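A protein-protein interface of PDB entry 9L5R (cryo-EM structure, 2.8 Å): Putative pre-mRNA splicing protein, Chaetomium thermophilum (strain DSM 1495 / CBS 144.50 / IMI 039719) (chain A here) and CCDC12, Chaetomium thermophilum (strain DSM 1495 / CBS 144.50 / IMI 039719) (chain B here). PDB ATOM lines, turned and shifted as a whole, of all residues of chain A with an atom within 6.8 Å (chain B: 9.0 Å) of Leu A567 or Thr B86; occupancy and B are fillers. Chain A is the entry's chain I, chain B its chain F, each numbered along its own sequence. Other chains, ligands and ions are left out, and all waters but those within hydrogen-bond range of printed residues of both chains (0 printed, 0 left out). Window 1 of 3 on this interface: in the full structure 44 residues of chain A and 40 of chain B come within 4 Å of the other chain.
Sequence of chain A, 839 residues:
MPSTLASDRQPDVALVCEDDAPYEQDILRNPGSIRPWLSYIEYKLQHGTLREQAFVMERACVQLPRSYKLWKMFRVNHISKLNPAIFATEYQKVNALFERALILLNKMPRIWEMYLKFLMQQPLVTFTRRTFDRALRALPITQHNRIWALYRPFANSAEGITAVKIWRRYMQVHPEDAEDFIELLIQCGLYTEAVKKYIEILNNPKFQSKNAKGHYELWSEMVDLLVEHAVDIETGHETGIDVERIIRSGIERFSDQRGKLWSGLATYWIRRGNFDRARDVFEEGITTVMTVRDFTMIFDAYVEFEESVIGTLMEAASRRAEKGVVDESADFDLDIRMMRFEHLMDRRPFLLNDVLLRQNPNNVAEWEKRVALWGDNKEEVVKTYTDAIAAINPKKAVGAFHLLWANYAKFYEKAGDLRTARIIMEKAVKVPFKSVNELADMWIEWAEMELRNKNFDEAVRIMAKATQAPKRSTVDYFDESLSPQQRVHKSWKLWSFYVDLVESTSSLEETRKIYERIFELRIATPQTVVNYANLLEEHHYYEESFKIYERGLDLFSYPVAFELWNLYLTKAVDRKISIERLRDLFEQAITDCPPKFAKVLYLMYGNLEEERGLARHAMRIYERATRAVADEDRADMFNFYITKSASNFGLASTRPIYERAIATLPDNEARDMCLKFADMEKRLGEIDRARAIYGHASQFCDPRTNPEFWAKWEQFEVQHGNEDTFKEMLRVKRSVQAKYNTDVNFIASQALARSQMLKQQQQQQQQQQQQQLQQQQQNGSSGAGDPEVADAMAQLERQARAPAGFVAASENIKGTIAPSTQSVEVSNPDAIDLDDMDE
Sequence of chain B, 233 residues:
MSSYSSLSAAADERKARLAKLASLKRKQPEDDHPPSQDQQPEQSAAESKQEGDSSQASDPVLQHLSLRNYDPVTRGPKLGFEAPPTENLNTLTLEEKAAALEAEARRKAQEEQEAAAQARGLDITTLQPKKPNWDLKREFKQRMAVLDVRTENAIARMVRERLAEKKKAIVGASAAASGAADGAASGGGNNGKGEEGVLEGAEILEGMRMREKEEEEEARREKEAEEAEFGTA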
ATOM      1  N   VAL A 530     -21.539  14.264  22.106  1.00  0.00           N
ATOM      2  CA  VAL A 530     -20.828  13.524  23.140  1.00  0.00           C
ATOM      3  C   VAL A 530     -21.709  13.312  24.367  1.00  0.00           C
ATOM      4  O   VAL A 530     -21.678  12.239  24.972  1.00  0.00           O
ATOM      5  CB  VAL A 530     -19.513  14.245  23.479  1.00  0.00           C
ATOM      6  CG1 VAL A 530     -18.845  13.615  24.668  1.00  0.00           C
ATOM      7  CG2 VAL A 530     -18.583  14.192  22.293  1.00  0.00           C
ATOM      8  N   ASN A 534     -22.782   9.755  25.692  1.00  0.00           N
ATOM      9  CA  ASN A 534     -22.446   9.431  27.070  1.00  0.00           C
ATOM     10  C   ASN A 534     -23.664   8.998  27.866  1.00  0.00           C
ATOM     11  O   ASN A 534     -23.550   8.108  28.709  1.00  0.00           O
ATOM     12  CB  ASN A 534     -21.786  10.632  27.745  1.00  0.00           C
ATOM     13  CG  ASN A 534     -20.309  10.726  27.443  1.00  0.00           C
ATOM     14  OD1 ASN A 534     -19.733   9.830  26.831  1.00  0.00           O
ATOM     15  ND2 ASN A 534     -19.686  11.817  27.867  1.00  0.00           N
ATOM     16  N   TYR A 549     -22.506   8.619  17.596  1.00  0.00           N
ATOM     17  CA  TYR A 549     -21.222   9.123  17.125  1.00  0.00           C
ATOM     18  C   TYR A 549     -21.157   9.162  15.605  1.00  0.00           C
ATOM     19  O   TYR A 549     -20.631  10.120  15.040  1.00  0.00           O
ATOM     20  CB  TYR A 549     -20.079   8.281  17.679  1.00  0.00           C
ATOM     21  CG  TYR A 549     -19.552   8.787  18.994  1.00  0.00           C
ATOM     22  CD1 TYR A 549     -19.027  10.058  19.103  1.00  0.00           C
ATOM     23  CD2 TYR A 549     -19.580   7.993  20.126  1.00  0.00           C
ATOM     24  CE1 TYR A 549     -18.549  10.528  20.299  1.00  0.00           C
ATOM     25  CE2 TYR A 549     -19.100   8.456  21.327  1.00  0.00           C
ATOM     26  CZ  TYR A 549     -18.588   9.724  21.406  1.00  0.00           C
ATOM     27  OH  TYR A 549     -18.108  10.195  22.601  1.00  0.00           O
ATOM     28  N   PHE A 562     -12.878  15.388  13.792  1.00  0.00           N
ATOM     29  CA  PHE A 562     -11.727  14.770  14.442  1.00  0.00           C
ATOM     30  C   PHE A 562     -11.899  14.683  15.948  1.00  0.00           C
ATOM     31  O   PHE A 562     -11.450  13.712  16.562  1.00  0.00           O
ATOM     32  CB  PHE A 562     -10.433  15.508  14.152  1.00  0.00           C
ATOM     33  CG  PHE A 562      -9.264  14.896  14.855  1.00  0.00           C
ATOM     34  CD1 PHE A 562      -8.867  13.609  14.555  1.00  0.00           C
ATOM     35  CD2 PHE A 562      -8.628  15.562  15.883  1.00  0.00           C
ATOM     36  CE1 PHE A 562      -7.820  13.026  15.216  1.00  0.00           C
ATOM     37  CE2 PHE A 562      -7.577  14.977  16.549  1.00  0.00           C
ATOM     38  CZ  PHE A 562      -7.174  13.711  16.212  1.00  0.00           C
ATOM     39  N   GLU A 563     -12.477  15.709  16.572  1.00  0.00           N
ATOM     40  CA  GLU A 563     -12.777  15.621  17.998  1.00  0.00           C
ATOM     41  C   GLU A 563     -13.718  14.457  18.256  1.00  0.00           C
ATOM     42  O   GLU A 563     -13.478  13.606  19.143  1.00  0.00           O
ATOM     43  CB  GLU A 563     -13.411  16.925  18.472  1.00  0.00           C
ATOM     44  CG  GLU A 563     -12.535  18.153  18.328  1.00  0.00           C
ATOM     45  CD  GLU A 563     -11.324  18.123  19.237  1.00  0.00           C
ATOM     46  OE1 GLU A 563     -11.411  17.537  20.336  1.00  0.00           O
ATOM     47  OE2 GLU A 563     -10.285  18.698  18.857  1.00  0.00           O
ATOM     48  N   LEU A 564     -14.758  14.367  17.423  1.00  0.00           N
ATOM     49  CA  LEU A 564     -15.662  13.224  17.542  1.00  0.00           C
ATOM     50  C   LEU A 564     -14.948  11.907  17.254  1.00  0.00           C
ATOM     51  O   LEU A 564     -15.254  10.888  17.875  1.00  0.00           O
ATOM     52  CB  LEU A 564     -16.867  13.375  16.622  1.00  0.00           C
ATOM     53  CG  LEU A 564     -18.014  14.249  17.115  1.00  0.00           C
ATOM     54  CD1 LEU A 564     -17.703  15.708  16.969  1.00  0.00           C
ATOM     55  CD2 LEU A 564     -19.249  13.908  16.371  1.00  0.00           C
ATOM     56  N   TRP A 565     -13.980  11.917  16.338  1.00  0.00           N
ATOM     57  CA  TRP A 565     -13.277  10.698  15.959  1.00  0.00           C
ATOM     58  C   TRP A 565     -12.365  10.221  17.073  1.00  0.00           C
ATOM     59  O   TRP A 565     -12.214   9.015  17.275  1.00  0.00           O
ATOM     60  CB  TRP A 565     -12.461  10.922  14.685  1.00  0.00           C
ATOM     61  CG  TRP A 565     -13.136  10.575  13.389  1.00  0.00           C
ATOM     62  CD1 TRP A 565     -13.277  11.384  12.310  1.00  0.00           C
ATOM     63  CD2 TRP A 565     -13.724   9.321  13.023  1.00  0.00           C
ATOM     64  NE1 TRP A 565     -13.931  10.731  11.307  1.00  0.00           N
ATOM     65  CE2 TRP A 565     -14.211   9.458  11.719  1.00  0.00           C
ATOM     66  CE3 TRP A 565     -13.888   8.098  13.674  1.00  0.00           C
ATOM     67  CZ2 TRP A 565     -14.847   8.428  11.056  1.00  0.00           C
ATOM     68  CZ3 TRP A 565     -14.523   7.081  13.013  1.00  0.00           C
ATOM     69  CH2 TRP A 565     -14.992   7.248  11.722  1.00  0.00           C
ATOM     70  N   ASN A 566     -11.722  11.155  17.778  1.00  0.00           N
ATOM     71  CA  ASN A 566     -10.932  10.863  18.968  1.00  0.00           C
ATOM     72  C   ASN A 566     -11.756  10.043  19.936  1.00  0.00           C
ATOM     73  O   ASN A 566     -11.423   8.882  20.244  1.00  0.00           O
ATOM     74  CB  ASN A 566     -10.493  12.137  19.687  1.00  0.00           C
ATOM     75  CG  ASN A 566      -9.228  12.715  19.136  1.00  0.00           C
ATOM     76  OD1 ASN A 566      -8.407  12.006  18.571  1.00  0.00           O
ATOM     77  ND2 ASN A 566      -9.033  14.007  19.345  1.00  0.00           N
ATOM     78  N   LEU A 567     -12.865  10.645  20.372  1.00  0.00           N
ATOM     79  CA  LEU A 567     -13.669   9.954  21.375  1.00  0.00           C
ATOM     80  C   LEU A 567     -14.277   8.654  20.851  1.00  0.00           C
ATOM     81  O   LEU A 567     -14.213   7.627  21.537  1.00  0.00           O
ATOM     82  CB  LEU A 567     -14.760  10.875  21.916  1.00  0.00           C
ATOM     83  CG  LEU A 567     -14.306  11.844  23.010  1.00  0.00           C
ATOM     84  CD1 LEU A 567     -13.482  13.015  22.495  1.00  0.00           C
ATOM     85  CD2 LEU A 567     -15.495  12.344  23.786  1.00  0.00           C
ATOM     86  N   TYR A 568     -14.796   8.663  19.623  1.00  0.00           N
ATOM     87  CA  TYR A 568     -15.459   7.491  19.067  1.00  0.00           C
ATOM     88  C   TYR A 568     -14.488   6.342  18.854  1.00  0.00           C
ATOM     89  O   TYR A 568     -14.820   5.192  19.146  1.00  0.00           O
ATOM     90  CB  TYR A 568     -16.136   7.869  17.752  1.00  0.00           C
ATOM     91  CG  TYR A 568     -16.841   6.749  17.023  1.00  0.00           C
ATOM     92  CD1 TYR A 568     -17.563   5.783  17.704  1.00  0.00           C
ATOM     93  CD2 TYR A 568     -16.796   6.674  15.646  1.00  0.00           C
ATOM     94  CE1 TYR A 568     -18.206   4.774  17.029  1.00  0.00           C
ATOM     95  CE2 TYR A 568     -17.438   5.674  14.964  1.00  0.00           C
ATOM     96  CZ  TYR A 568     -18.140   4.727  15.659  1.00  0.00           C
ATOM     97  OH  TYR A 568     -18.780   3.724  14.978  1.00  0.00           O
ATOM     98  N   LEU A 569     -13.290   6.622  18.348  1.00  0.00           N
ATOM     99  CA  LEU A 569     -12.365   5.543  18.042  1.00  0.00           C
ATOM    100  C   LEU A 569     -11.798   4.933  19.311  1.00  0.00           C
ATOM    101  O   LEU A 569     -11.645   3.705  19.391  1.00  0.00           O
ATOM    102  CB  LEU A 569     -11.254   6.049  17.132  1.00  0.00           C
ATOM    103  CG  LEU A 569     -11.646   6.062  15.658  1.00  0.00           C
ATOM    104  CD1 LEU A 569     -10.506   6.556  14.801  1.00  0.00           C
ATOM    105  CD2 LEU A 569     -12.080   4.685  15.223  1.00  0.00           C
ATOM    106  N   THR A 570     -11.512   5.761  20.327  1.00  0.00           N
ATOM    107  CA  THR A 570     -11.089   5.181  21.600  1.00  0.00           C
ATOM    108  C   THR A 570     -12.189   4.325  22.214  1.00  0.00           C
ATOM    109  O   THR A 570     -11.921   3.211  22.680  1.00  0.00           O
ATOM    110  CB  THR A 570     -10.659   6.270  22.574  1.00  0.00           C
ATOM    111  OG1 THR A 570     -11.731   7.198  22.765  1.00  0.00           O
ATOM    112  CG2 THR A 570      -9.444   6.989  22.043  1.00  0.00           C
ATOM    113  N   LYS A 571     -13.438   4.803  22.184  1.00  0.00           N
ATOM    114  CA  LYS A 571     -14.524   4.032  22.781  1.00  0.00           C
ATOM    115  C   LYS A 571     -14.803   2.749  22.008  1.00  0.00           C
ATOM    116  O   LYS A 571     -15.114   1.718  22.609  1.00  0.00           O
ATOM    117  CB  LYS A 571     -15.781   4.888  22.877  1.00  0.00           C
ATOM    118  CG  LYS A 571     -15.658   6.002  23.882  1.00  0.00           C
ATOM    119  CD  LYS A 571     -17.003   6.484  24.342  1.00  0.00           C
ATOM    120  CE  LYS A 571     -16.890   7.852  24.965  1.00  0.00           C
ATOM    121  NZ  LYS A 571     -15.513   8.104  25.453  1.00  0.00           N
ATOM    122  N   ALA A 572     -14.672   2.781  20.684  1.00  0.00           N
ATOM    123  CA  ALA A 572     -14.927   1.582  19.894  1.00  0.00           C
ATOM    124  C   ALA A 572     -13.838   0.539  20.097  1.00  0.00           C
ATOM    125  O   ALA A 572     -14.133  -0.660  20.201  1.00  0.00           O
ATOM    126  CB  ALA A 572     -15.051   1.946  18.416  1.00  0.00           C
ATOM    127  N   GLY B  80     -18.145  23.867  25.648  1.00  0.00           N
ATOM    128  CA  GLY B  80     -16.993  23.005  25.471  1.00  0.00           C
ATOM    129  C   GLY B  80     -15.694  23.734  25.239  1.00  0.00           C
ATOM    130  O   GLY B  80     -14.638  23.096  25.189  1.00  0.00           O
ATOM    131  N   GLU B  82     -14.505  25.908  27.402  1.00  0.00           N
ATOM    132  CA  GLU B  82     -13.903  25.962  28.727  1.00  0.00           C
ATOM    133  C   GLU B  82     -13.738  24.576  29.336  1.00  0.00           C
ATOM    134  O   GLU B  82     -12.647  24.219  29.785  1.00  0.00           O
ATOM    135  CB  GLU B  82     -14.753  26.840  29.644  1.00  0.00           C
ATOM    136  CG  GLU B  82     -15.052  28.206  29.068  1.00  0.00           C
ATOM    137  CD  GLU B  82     -16.364  28.764  29.566  1.00  0.00           C
ATOM    138  OE1 GLU B  82     -16.945  28.171  30.499  1.00  0.00           O
ATOM    139  OE2 GLU B  82     -16.810  29.798  29.030  1.00  0.00           O
ATOM    140  N   ALA B  83     -14.806  23.786  29.351  1.00  0.00           N
ATOM    141  CA  ALA B  83     -14.783  22.452  29.946  1.00  0.00           C
ATOM    142  C   ALA B  83     -15.065  21.414  28.874  1.00  0.00           C
ATOM    143  O   ALA B  83     -16.238  21.101  28.604  1.00  0.00           O
ATOM    144  CB  ALA B  83     -15.802  22.346  31.077  1.00  0.00           C
ATOM    145  N   PRO B  84     -14.036  20.865  28.229  1.00  0.00           N
ATOM    146  CA  PRO B  84     -14.266  19.801  27.261  1.00  0.00           C
ATOM    147  C   PRO B  84     -14.756  18.544  27.953  1.00  0.00           C
ATOM    148  O   PRO B  84     -14.449  18.312  29.134  1.00  0.00           O
ATOM    149  CB  PRO B  84     -12.877  19.584  26.634  1.00  0.00           C
ATOM    150  CG  PRO B  84     -12.102  20.799  26.968  1.00  0.00           C
ATOM    151  CD  PRO B  84     -12.626  21.276  28.276  1.00  0.00           C
ATOM    152  N   PRO B  85     -15.527  17.703  27.263  1.00  0.00           N
ATOM    153  CA  PRO B  85     -15.871  16.386  27.808  1.00  0.00           C
ATOM    154  C   PRO B  85     -14.692  15.433  27.933  1.00  0.00           C
ATOM    155  O   PRO B  85     -14.798  14.437  28.657  1.00  0.00           O
ATOM    156  CB  PRO B  85     -16.900  15.851  26.803  1.00  0.00           C
ATOM    157  CG  PRO B  85     -16.719  16.631  25.577  1.00  0.00           C
ATOM    158  CD  PRO B  85     -16.075  17.926  25.917  1.00  0.00           C
ATOM    159  N   THR B  86     -13.579  15.719  27.260  1.00  0.00           N
ATOM    160  CA  THR B  86     -12.341  14.987  27.472  1.00  0.00           C
ATOM    161  C   THR B  86     -11.811  15.124  28.891  1.00  0.00           C
ATOM    162  O   THR B  86     -11.096  14.229  29.356  1.00  0.00           O
ATOM    163  CB  THR B  86     -11.274  15.459  26.482  1.00  0.00           C
ATOM    164  OG1 THR B  86     -10.907  16.810  26.783  1.00  0.00           O
ATOM    165  CG2 THR B  86     -11.802  15.394  25.064  1.00  0.00           C
ATOM    166  N   GLU B  87     -12.135  16.220  29.584  1.00  0.00           N
ATOM    167  CA  GLU B  87     -11.869  16.291  31.016  1.00  0.00           C
ATOM    168  C   GLU B  87     -12.711  15.277  31.778  1.00  0.00           C
ATOM    169  O   GLU B  87     -12.198  14.557  32.644  1.00  0.00           O
ATOM    170  CB  GLU B  87     -12.149  17.698  31.537  1.00  0.00           C
ATOM    171  CG  GLU B  87     -11.259  18.778  30.961  1.00  0.00           C
ATOM    172  CD  GLU B  87     -11.411  20.095  31.697  1.00  0.00           C
ATOM    173  OE1 GLU B  87     -12.097  20.112  32.740  1.00  0.00           O
ATOM    174  OE2 GLU B  87     -10.848  21.110  31.238  1.00  0.00           O
ATOM    175  N   ASN B  88     -14.002  15.197  31.457  1.00  0.00           N
ATOM    176  CA  ASN B  88     -14.918  14.305  32.155  1.00  0.00           C
ATOM    177  C   ASN B  88     -14.706  12.838  31.806  1.00  0.00           C
ATOM    178  O   ASN B  88     -15.276  11.978  32.485  1.00  0.00           O
ATOM    179  CB  ASN B  88     -16.362  14.700  31.846  1.00  0.00           C
ATOM    180  CG  ASN B  88     -16.708  16.087  32.354  1.00  0.00           C
ATOM    181  OD1 ASN B  88     -16.978  16.997  31.572  1.00  0.00           O
ATOM    182  ND2 ASN B  88     -16.706  16.253  33.671  1.00  0.00           N
ATOM    183  N   LEU B  89     -13.928  12.533  30.768  1.00  0.00           N
ATOM    184  CA  LEU B  89     -13.653  11.142  30.434  1.00  0.00           C
ATOM    185  C   LEU B  89     -12.830  10.454  31.517  1.00  0.00           C
ATOM    186  O   LEU B  89     -12.080  11.088  32.263  1.00  0.00           O
ATOM    187  CB  LEU B  89     -12.907  11.027  29.106  1.00  0.00           C
ATOM    188  CG  LEU B  89     -13.635  11.450  27.838  1.00  0.00           C
ATOM    189  CD1 LEU B  89     -12.686  11.387  26.654  1.00  0.00           C
ATOM    190  CD2 LEU B  89     -14.855  10.580  27.621  1.00  0.00           C
ATOM    191  N   ASN B  90     -12.988   9.134  31.593  1.00  0.00           N
ATOM    192  CA  ASN B  90     -12.210   8.285  32.484  1.00  0.00           C
ATOM    193  C   ASN B  90     -11.064   7.566  31.779  1.00  0.00           C
ATOM    194  O   ASN B  90     -10.349   6.787  32.414  1.00  0.00           O
ATOM    195  CB  ASN B  90     -13.136   7.283  33.191  1.00  0.00           C
ATOM    196  CG  ASN B  90     -13.832   6.302  32.231  1.00  0.00           C
ATOM    197  OD1 ASN B  90     -13.567   6.256  31.030  1.00  0.00           O
ATOM    198  ND2 ASN B  90     -14.740   5.508  32.785  1.00  0.00           N
ATOM    199  N   THR B  91     -10.882   7.802  30.486  1.00  0.00           N
ATOM    200  CA  THR B  91      -9.918   7.076  29.674  1.00  0.00           C
ATOM    201  C   THR B  91      -9.026   8.055  28.920  1.00  0.00           C
ATOM    202  O   THR B  91      -9.098   9.272  29.103  1.00  0.00           O
ATOM    203  CB  THR B  91     -10.629   6.136  28.699  1.00  0.00           C
ATOM    204  OG1 THR B  91      -9.657   5.413  27.936  1.00  0.00           O
ATOM    205  CG2 THR B  91     -11.522   6.924  27.759  1.00  0.00           C
ATOM    206  N   LEU B  92      -8.176   7.501  28.061  1.00  0.00           N
ATOM    207  CA  LEU B  92      -7.243   8.280  27.262  1.00  0.00           C
ATOM    208  C   LEU B  92      -7.796   8.473  25.860  1.00  0.00           C
ATOM    209  O   LEU B  92      -8.254   7.519  25.225  1.00  0.00           O
ATOM    210  CB  LEU B  92      -5.877   7.596  27.178  1.00  0.00           C
ATOM    211  CG  LEU B  92      -4.896   7.712  28.345  1.00  0.00           C
ATOM    212  CD1 LEU B  92      -5.257   6.764  29.478  1.00  0.00           C
ATOM    213  CD2 LEU B  92      -3.482   7.458  27.859  1.00  0.00           C
ATOM    214  N   THR B  93      -7.735   9.710  25.374  1.00  0.00           N
ATOM    215  CA  THR B  93      -8.143   9.999  24.010  1.00  0.00           C
ATOM    216  C   THR B  93      -7.100   9.463  23.033  1.00  0.00           C
ATOM    217  O   THR B  93      -6.058   8.929  23.418  1.00  0.00           O
ATOM    218  CB  THR B  93      -8.343  11.498  23.819  1.00  0.00           C
ATOM    219  OG1 THR B  93      -7.122  12.181  24.112  1.00  0.00           O
ATOM    220  CG2 THR B  93      -9.416  12.003  24.754  1.00  0.00           C
ATOM    221  N   LEU B  94      -7.380   9.638  21.744  1.00  0.00           N
ATOM    222  CA  LEU B  94      -6.583   8.993  20.709  1.00  0.00           C
ATOM    223  C   LEU B  94      -5.212   9.658  20.589  1.00  0.00           C
ATOM    224  O   LEU B  94      -4.193   8.975  20.331  1.00  0.00           O
ATOM    225  CB  LEU B  94      -7.357   9.066  19.397  1.00  0.00           C
ATOM    226  CG  LEU B  94      -7.072   8.170  18.207  1.00  0.00           C
ATOM    227  CD1 LEU B  94      -7.546   6.781  18.566  1.00  0.00           C
ATOM    228  CD2 LEU B  94      -7.788   8.680  16.985  1.00  0.00           C
ATOM    229  N   GLU B  95      -5.175  10.979  20.875  1.00  0.00           N
ATOM    230  CA  GLU B  95      -4.014  11.865  20.755  1.00  0.00           C
ATOM    231  C   GLU B  95      -3.114  11.831  21.996  1.00  0.00           C
ATOM    232  O   GLU B  95      -1.883  11.750  21.858  1.00  0.00           O
ATOM    233  CB  GLU B  95      -4.480  13.291  20.465  1.00  0.00           C
ATOM    234  CG  GLU B  95      -5.482  13.837  21.465  1.00  0.00           C
ATOM    235  CD  GLU B  95      -5.947  15.228  21.119  1.00  0.00           C
ATOM    236  OE1 GLU B  95      -5.491  15.765  20.089  1.00  0.00           O
ATOM    237  OE2 GLU B  95      -6.768  15.787  21.876  1.00  0.00           O
ATOM    238  N   GLU B  96      -3.701  11.726  23.195  1.00  0.00           N
ATOM    239  CA  GLU B  96      -2.932  11.369  24.389  1.00  0.00           C
ATOM    240  C   GLU B  96      -2.350   9.965  24.257  1.00  0.00           C
ATOM    241  O   GLU B  96      -1.138   9.751  24.398  1.00  0.00           O
ATOM    242  CB  GLU B  96      -3.830  11.458  25.622  1.00  0.00           C
ATOM    243  CG  GLU B  96      -4.393  12.835  25.887  1.00  0.00           C
ATOM    244  CD  GLU B  96      -5.438  12.827  26.983  1.00  0.00           C
ATOM    245  OE1 GLU B  96      -5.782  11.727  27.465  1.00  0.00           O
ATOM    246  OE2 GLU B  96      -5.916  13.916  27.359  1.00  0.00           O
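Printed residues of chain A that touch a printed residue of chain B: Val A530, Asn A566, Leu A567, Thr A570 and Lys A571.
Hydrophobic or aromatic side chains of chain A within 4 Å of the printed part of chain B: Val A530 and Leu A567.
Of the 16 printed residues of chain B, 7 touch a printed residue of chain A.
Among the printed residues, merely in contact across the chains: Asn A566 with Leu B94, Lys A571 with Leu B89, Thr A570 with Leu B94, Thr A570 with Leu B92, Thr A570 with Thr B93, Val A530 with Pro B85, Asn A566 with Glu B95 and Leu A567 with Thr B86.
OG1 of Thr A570 lies within hydrogen-bond range of O of Asn A566 (3.0 Å).
The backbone carbonyl oxygen (O) of Leu A567 lies within hydrogen-bond range of the side-chain hydroxyl (OG1) of Thr A570 (2.8 Å).
Of the printed residues of chain B, Leu A567 touches Thr B86 (3.9 Å).
Of the printed residues of chain A, Pro B85 touches Val A530.
Printed residues of chain A within 4 Å of Thr B93: Thr A570 (3.5 Å).
Of the printed residues of chain A, Leu B94 touches Asn A566 (3.2 Å) and Thr A570 (3.4 Å).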
